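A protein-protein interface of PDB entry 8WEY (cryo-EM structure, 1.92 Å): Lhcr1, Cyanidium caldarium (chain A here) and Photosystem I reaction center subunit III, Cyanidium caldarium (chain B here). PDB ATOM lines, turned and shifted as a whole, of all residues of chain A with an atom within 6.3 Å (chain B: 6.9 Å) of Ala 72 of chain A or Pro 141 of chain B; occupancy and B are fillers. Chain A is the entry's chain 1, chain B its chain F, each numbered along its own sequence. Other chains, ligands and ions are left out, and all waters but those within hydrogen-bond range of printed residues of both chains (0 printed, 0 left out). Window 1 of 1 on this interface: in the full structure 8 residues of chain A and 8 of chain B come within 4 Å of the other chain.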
ATOM      1  N   ASN A  53     -14.998  10.904   2.118  1.00  0.00           N
ATOM      2  CA  ASN A  53     -14.088  11.450   3.165  1.00  0.00           C
ATOM      3  C   ASN A  53     -13.222  10.336   3.771  1.00  0.00           C
ATOM      4  O   ASN A  53     -12.138  10.669   4.293  1.00  0.00           O
ATOM      5  CB  ASN A  53     -14.861  12.213   4.244  1.00  0.00           C
ATOM      6  CG  ASN A  53     -15.564  13.441   3.705  1.00  0.00           C
ATOM      7  OD1 ASN A  53     -15.061  14.118   2.809  1.00  0.00           O
ATOM      8  ND2 ASN A  53     -16.726  13.746   4.253  1.00  0.00           N
ATOM      9  N   ARG A  68     -23.374   7.491   6.035  1.00  0.00           N
ATOM     10  CA  ARG A  68     -22.510   8.636   5.629  1.00  0.00           C
ATOM     11  C   ARG A  68     -22.352   9.597   6.817  1.00  0.00           C
ATOM     12  O   ARG A  68     -22.559  10.810   6.644  1.00  0.00           O
ATOM     13  CB  ARG A  68     -23.072   9.321   4.376  1.00  0.00           C
ATOM     14  CG  ARG A  68     -23.027   8.464   3.118  1.00  0.00           C
ATOM     15  CD  ARG A  68     -21.608   8.177   2.660  1.00  0.00           C
ATOM     16  NE  ARG A  68     -21.546   7.744   1.268  1.00  0.00           N
ATOM     17  CZ  ARG A  68     -21.629   8.539   0.198  1.00  0.00           C
ATOM     18  NH1 ARG A  68     -21.791   9.850   0.331  1.00  0.00           N
ATOM     19  NH2 ARG A  68     -21.547   8.006  -1.014  1.00  0.00           N
ATOM     20  N   LEU A  69     -21.992   9.059   7.984  1.00  0.00           N
ATOM     21  CA  LEU A  69     -21.661   9.834   9.209  1.00  0.00           C
ATOM     22  C   LEU A  69     -20.316  10.552   9.018  1.00  0.00           C
ATOM     23  O   LEU A  69     -20.120  11.598   9.658  1.00  0.00           O
ATOM     24  CB  LEU A  69     -21.639   8.885  10.414  1.00  0.00           C
ATOM     25  CG  LEU A  69     -22.986   8.255  10.774  1.00  0.00           C
ATOM     26  CD1 LEU A  69     -22.807   7.088  11.734  1.00  0.00           C
ATOM     27  CD2 LEU A  69     -23.931   9.288  11.369  1.00  0.00           C
ATOM     28  N   SER A  70     -19.444  10.030   8.148  1.00  0.00           N
ATOM     29  CA  SER A  70     -18.150  10.646   7.742  1.00  0.00           C
ATOM     30  C   SER A  70     -18.375  11.934   6.932  1.00  0.00           C
ATOM     31  O   SER A  70     -17.418  12.727   6.835  1.00  0.00           O
ATOM     32  CB  SER A  70     -17.293   9.665   6.980  1.00  0.00           C
ATOM     33  OG  SER A  70     -17.947   9.226   5.796  1.00  0.00           O
ATOM     34  N   ASP A  71     -19.568  12.126   6.353  1.00  0.00           N
ATOM     35  CA  ASP A  71     -20.009  13.407   5.729  1.00  0.00           C
ATOM     36  C   ASP A  71     -20.507  14.369   6.818  1.00  0.00           C
ATOM     37  O   ASP A  71     -20.229  15.579   6.711  1.00  0.00           O
ATOM     38  CB  ASP A  71     -21.094  13.181   4.671  1.00  0.00           C
ATOM     39  CG  ASP A  71     -20.684  12.272   3.521  1.00  0.00           C
ATOM     40  OD1 ASP A  71     -19.533  11.780   3.532  1.00  0.00           O
ATOM     41  OD2 ASP A  71     -21.522  12.059   2.617  1.00  0.00           O
ATOM     42  N   ALA A  72     -21.231  13.848   7.815  1.00  0.00           N
ATOM     43  CA  ALA A  72     -21.868  14.614   8.911  1.00  0.00           C
ATOM     44  C   ALA A  72     -20.815  15.119   9.905  1.00  0.00           C
ATOM     45  O   ALA A  72     -20.974  16.254  10.393  1.00  0.00           O
ATOM     46  CB  ALA A  72     -22.902  13.758   9.601  1.00  0.00           C
ATOM     47  N   PHE A  73     -19.801  14.300  10.209  1.00  0.00           N
ATOM     48  CA  PHE A  73     -18.741  14.584  11.216  1.00  0.00           C
ATOM     49  C   PHE A  73     -17.360  14.476  10.561  1.00  0.00           C
ATOM     50  O   PHE A  73     -17.219  13.743   9.564  1.00  0.00           O
ATOM     51  CB  PHE A  73     -18.879  13.629  12.404  1.00  0.00           C
ATOM     52  CG  PHE A  73     -20.233  13.664  13.069  1.00  0.00           C
ATOM     53  CD1 PHE A  73     -20.503  14.564  14.089  1.00  0.00           C
ATOM     54  CD2 PHE A  73     -21.250  12.816  12.655  1.00  0.00           C
ATOM     55  CE1 PHE A  73     -21.753  14.603  14.690  1.00  0.00           C
ATOM     56  CE2 PHE A  73     -22.501  12.860  13.252  1.00  0.00           C
ATOM     57  CZ  PHE A  73     -22.751  13.754  14.267  1.00  0.00           C
ATOM     58  N   ASP A  74     -16.378  15.200  11.105  1.00  0.00           N
ATOM     59  CA  ASP A  74     -14.960  15.203  10.640  1.00  0.00           C
ATOM     60  C   ASP A  74     -14.370  13.813  10.902  1.00  0.00           C
ATOM     61  O   ASP A  74     -14.504  13.330  12.041  1.00  0.00           O
ATOM     62  CB  ASP A  74     -14.119  16.276  11.339  1.00  0.00           C
ATOM     63  CG  ASP A  74     -14.629  17.697  11.167  1.00  0.00           C
ATOM     64  OD1 ASP A  74     -15.065  18.035  10.045  1.00  0.00           O
ATOM     65  OD2 ASP A  74     -14.587  18.457  12.157  1.00  0.00           O
ATOM     66  N   LEU A  78     -14.065  11.095  14.305  1.00  0.00           N
ATOM     67  CA  LEU A  78     -14.715   9.756  14.253  1.00  0.00           C
ATOM     68  C   LEU A  78     -13.650   8.672  14.457  1.00  0.00           C
ATOM     69  O   LEU A  78     -13.878   7.781  15.297  1.00  0.00           O
ATOM     70  CB  LEU A  78     -15.425   9.559  12.908  1.00  0.00           C
ATOM     71  CG  LEU A  78     -16.617  10.468  12.627  1.00  0.00           C
ATOM     72  CD1 LEU A  78     -17.191  10.194  11.241  1.00  0.00           C
ATOM     73  CD2 LEU A  78     -17.700  10.287  13.687  1.00  0.00           C
ATOM     74  N   TYR A 148     -14.399  18.666  20.344  1.00  0.00           N
ATOM     75  CA  TYR A 148     -14.570  18.378  18.897  1.00  0.00           C
ATOM     76  C   TYR A 148     -14.189  19.623  18.080  1.00  0.00           C
ATOM     77  O   TYR A 148     -13.637  19.469  16.971  1.00  0.00           O
ATOM     78  CB  TYR A 148     -15.984  17.847  18.641  1.00  0.00           C
ATOM     79  CG  TYR A 148     -16.319  17.536  17.205  1.00  0.00           C
ATOM     80  CD1 TYR A 148     -15.358  17.177  16.269  1.00  0.00           C
ATOM     81  CD2 TYR A 148     -17.638  17.539  16.795  1.00  0.00           C
ATOM     82  CE1 TYR A 148     -15.689  16.953  14.942  1.00  0.00           C
ATOM     83  CE2 TYR A 148     -17.993  17.272  15.480  1.00  0.00           C
ATOM     84  CZ  TYR A 148     -17.013  16.987  14.547  1.00  0.00           C
ATOM     85  OH  TYR A 148     -17.363  16.752  13.252  1.00  0.00           O
ATOM     86  N   TYR B 121     -21.762  28.746  17.229  1.00  0.00           N
ATOM     87  CA  TYR B 121     -22.317  28.584  15.866  1.00  0.00           C
ATOM     88  C   TYR B 121     -22.536  29.962  15.241  1.00  0.00           C
ATOM     89  O   TYR B 121     -22.202  30.129  14.060  1.00  0.00           O
ATOM     90  CB  TYR B 121     -23.617  27.778  15.853  1.00  0.00           C
ATOM     91  CG  TYR B 121     -24.178  27.590  14.469  1.00  0.00           C
ATOM     92  CD1 TYR B 121     -23.684  26.609  13.623  1.00  0.00           C
ATOM     93  CD2 TYR B 121     -25.164  28.431  13.979  1.00  0.00           C
ATOM     94  CE1 TYR B 121     -24.181  26.445  12.339  1.00  0.00           C
ATOM     95  CE2 TYR B 121     -25.681  28.275  12.704  1.00  0.00           C
ATOM     96  CZ  TYR B 121     -25.186  27.281  11.879  1.00  0.00           C
ATOM     97  OH  TYR B 121     -25.692  27.149  10.621  1.00  0.00           O
ATOM     98  N   LEU B 138     -29.465  25.689   8.510  1.00  0.00           N
ATOM     99  CA  LEU B 138     -28.316  25.348   9.387  1.00  0.00           C
ATOM    100  C   LEU B 138     -27.265  24.585   8.581  1.00  0.00           C
ATOM    101  O   LEU B 138     -27.647  23.724   7.775  1.00  0.00           O
ATOM    102  CB  LEU B 138     -28.782  24.496  10.571  1.00  0.00           C
ATOM    103  CG  LEU B 138     -29.626  25.200  11.632  1.00  0.00           C
ATOM    104  CD1 LEU B 138     -29.777  24.311  12.857  1.00  0.00           C
ATOM    105  CD2 LEU B 138     -29.026  26.535  12.035  1.00  0.00           C
ATOM    106  N   ASP B 139     -25.992  24.914   8.799  1.00  0.00           N
ATOM    107  CA  ASP B 139     -24.839  24.034   8.486  1.00  0.00           C
ATOM    108  C   ASP B 139     -24.806  22.963   9.582  1.00  0.00           C
ATOM    109  O   ASP B 139     -24.191  23.219  10.634  1.00  0.00           O
ATOM    110  CB  ASP B 139     -23.542  24.844   8.382  1.00  0.00           C
ATOM    111  CG  ASP B 139     -22.335  24.031   7.944  1.00  0.00           C
ATOM    112  OD1 ASP B 139     -22.187  22.882   8.414  1.00  0.00           O
ATOM    113  OD2 ASP B 139     -21.547  24.550   7.128  1.00  0.00           O
ATOM    114  N   LEU B 140     -25.473  21.829   9.359  1.00  0.00           N
ATOM    115  CA  LEU B 140     -25.692  20.784  10.399  1.00  0.00           C
ATOM    116  C   LEU B 140     -24.359  20.224  10.890  1.00  0.00           C
ATOM    117  O   LEU B 140     -24.179  20.105  12.100  1.00  0.00           O
ATOM    118  CB  LEU B 140     -26.615  19.681   9.877  1.00  0.00           C
ATOM    119  CG  LEU B 140     -28.080  20.074   9.709  1.00  0.00           C
ATOM    120  CD1 LEU B 140     -28.878  18.902   9.158  1.00  0.00           C
ATOM    121  CD2 LEU B 140     -28.678  20.569  11.020  1.00  0.00           C
ATOM    122  N   PRO B 141     -23.392  19.865  10.012  1.00  0.00           N
ATOM    123  CA  PRO B 141     -22.069  19.441  10.474  1.00  0.00           C
ATOM    124  C   PRO B 141     -21.415  20.424  11.452  1.00  0.00           C
ATOM    125  O   PRO B 141     -20.894  19.973  12.459  1.00  0.00           O
ATOM    126  CB  PRO B 141     -21.247  19.359   9.178  1.00  0.00           C
ATOM    127  CG  PRO B 141     -22.273  18.995   8.138  1.00  0.00           C
ATOM    128  CD  PRO B 141     -23.519  19.755   8.549  1.00  0.00           C
ATOM    129  N   MET B 142     -21.471  21.725  11.148  1.00  0.00           N
ATOM    130  CA  MET B 142     -20.874  22.781  12.007  1.00  0.00           C
ATOM    131  C   MET B 142     -21.702  22.932  13.284  1.00  0.00           C
ATOM    132  O   MET B 142     -21.084  23.072  14.347  1.00  0.00           O
ATOM    133  CB  MET B 142     -20.760  24.124  11.276  1.00  0.00           C
ATOM    134  CG  MET B 142     -19.667  24.120  10.219  1.00  0.00           C
ATOM    135  SD  MET B 142     -18.039  23.605  10.835  1.00  0.00           S
ATOM    136  CE  MET B 142     -17.760  24.828  12.113  1.00  0.00           C
ATOM    137  N   ALA B 143     -23.032  22.876  13.191  1.00  0.00           N
ATOM    138  CA  ALA B 143     -23.938  22.910  14.363  1.00  0.00           C
ATOM    139  C   ALA B 143     -23.577  21.758  15.311  1.00  0.00           C
ATOM    140  O   ALA B 143     -23.410  22.012  16.516  1.00  0.00           O
ATOM    141  CB  ALA B 143     -25.384  22.839  13.928  1.00  0.00           C
ATOM    142  N   PHE B 144     -23.438  20.540  14.780  1.00  0.00           N
ATOM    143  CA  PHE B 144     -23.063  19.329  15.559  1.00  0.00           C
ATOM    144  C   PHE B 144     -21.696  19.533  16.212  1.00  0.00           C
ATOM    145  O   PHE B 144     -21.550  19.160  17.388  1.00  0.00           O
ATOM    146  CB  PHE B 144     -23.019  18.067  14.695  1.00  0.00           C
ATOM    147  CG  PHE B 144     -24.301  17.694  13.995  1.00  0.00           C
ATOM    148  CD1 PHE B 144     -25.543  18.019  14.525  1.00  0.00           C
ATOM    149  CD2 PHE B 144     -24.258  16.987  12.801  1.00  0.00           C
ATOM    150  CE1 PHE B 144     -26.710  17.659  13.865  1.00  0.00           C
ATOM    151  CE2 PHE B 144     -25.426  16.627  12.145  1.00  0.00           C
ATOM    152  CZ  PHE B 144     -26.650  16.963  12.680  1.00  0.00           C
ATOM    153  N   LYS B 145     -20.737  20.106  15.481  1.00  0.00           N
ATOM    154  CA  LYS B 145     -19.354  20.326  15.979  1.00  0.00           C
ATOM    155  C   LYS B 145     -19.409  21.169  17.257  1.00  0.00           C
ATOM    156  O   LYS B 145     -18.788  20.766  18.262  1.00  0.00           O
ATOM    157  CB  LYS B 145     -18.466  20.985  14.919  1.00  0.00           C
ATOM    158  CG  LYS B 145     -17.011  21.173  15.331  1.00  0.00           C
ATOM    159  CD  LYS B 145     -16.207  22.036  14.383  1.00  0.00           C
ATOM    160  CE  LYS B 145     -15.547  21.241  13.277  1.00  0.00           C
ATOM    161  NZ  LYS B 145     -14.294  20.598  13.743  1.00  0.00           N
ATOM    162  N   TYR B 146     -20.126  22.290  17.216  1.00  0.00           N
ATOM    163  CA  TYR B 146     -20.238  23.242  18.350  1.00  0.00           C
ATOM    164  C   TYR B 146     -21.105  22.635  19.451  1.00  0.00           C
ATOM    165  O   TYR B 146     -20.742  22.807  20.620  1.00  0.00           O
ATOM    166  CB  TYR B 146     -20.730  24.599  17.854  1.00  0.00           C
ATOM    167  CG  TYR B 146     -19.733  25.260  16.940  1.00  0.00           C
ATOM    168  CD1 TYR B 146     -18.429  25.481  17.360  1.00  0.00           C
ATOM    169  CD2 TYR B 146     -20.070  25.623  15.646  1.00  0.00           C
ATOM    170  CE1 TYR B 146     -17.493  26.075  16.532  1.00  0.00           C
ATOM    171  CE2 TYR B 146     -19.140  26.212  14.802  1.00  0.00           C
ATOM    172  CZ  TYR B 146     -17.849  26.439  15.246  1.00  0.00           C
ATOM    173  OH  TYR B 146     -16.920  27.019  14.431  1.00  0.00           O
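Among the printed residues, pairs that only touch across the chains: Ala 72 of chain A with Pro 141 of chain B (3.3 Å) and Phe 73 of chain A with Phe 144 of chain B (3.7 Å).
Of the 10 printed residues of chain B, 3 touch a printed residue of chain A.
Among the printed residues, 4 pairs touch across the chains.
The side-chain carboxylate (OD2) of Asp 74 of chain A is in salt-bridge range of the side-chain amino group (NZ) of Lys 145 of chain B, at 2.7 Å.
The backbone carbonyl oxygen of Tyr 148 of chain A lies within hydrogen-bond range of the side-chain amino group of Lys 145 of chain B (3.5 Å).
Asp 71 of chain A touches none of the printed residues of chain B.
Ala 72 of chain A touches one residue of chain B.
Of the printed residues of chain B, Phe 73 of chain A touches Phe 144 (3.7 Å).
Printed residues of chain B within 4 Å of Asp 74 of chain A: Lys 145 (2.7 Å).
Printed residues of chain B within 4 Å of Tyr 148 of chain A: Lys 145 (3.4 Å).
Pro 141 of chain B touches just one residue of chain A: Ala 72.
Met 142 of chain B touches none of the printed residues of chain A.
Printed residues of chain A within 4 Å of Phe 144 of chain B: Phe 73 (3.7 Å).
Of the printed residues of chain A, Lys 145 of chain B touches Asp 74 (2.7 Å) and Tyr 148 (3.4 Å).
The nearest residue of chain B that does not touch Ala 72 of chain A is Phe 144 of chain B (4.1 Å).
The nearest printed residue of chain A that does not touch Phe 144 of chain B is Ala 72 of chain A (4.1 Å).
OH of Tyr 148 of chain A sits at hydrogen-bond distance from N of Asp 74 of chain A, at 2.8 Å.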
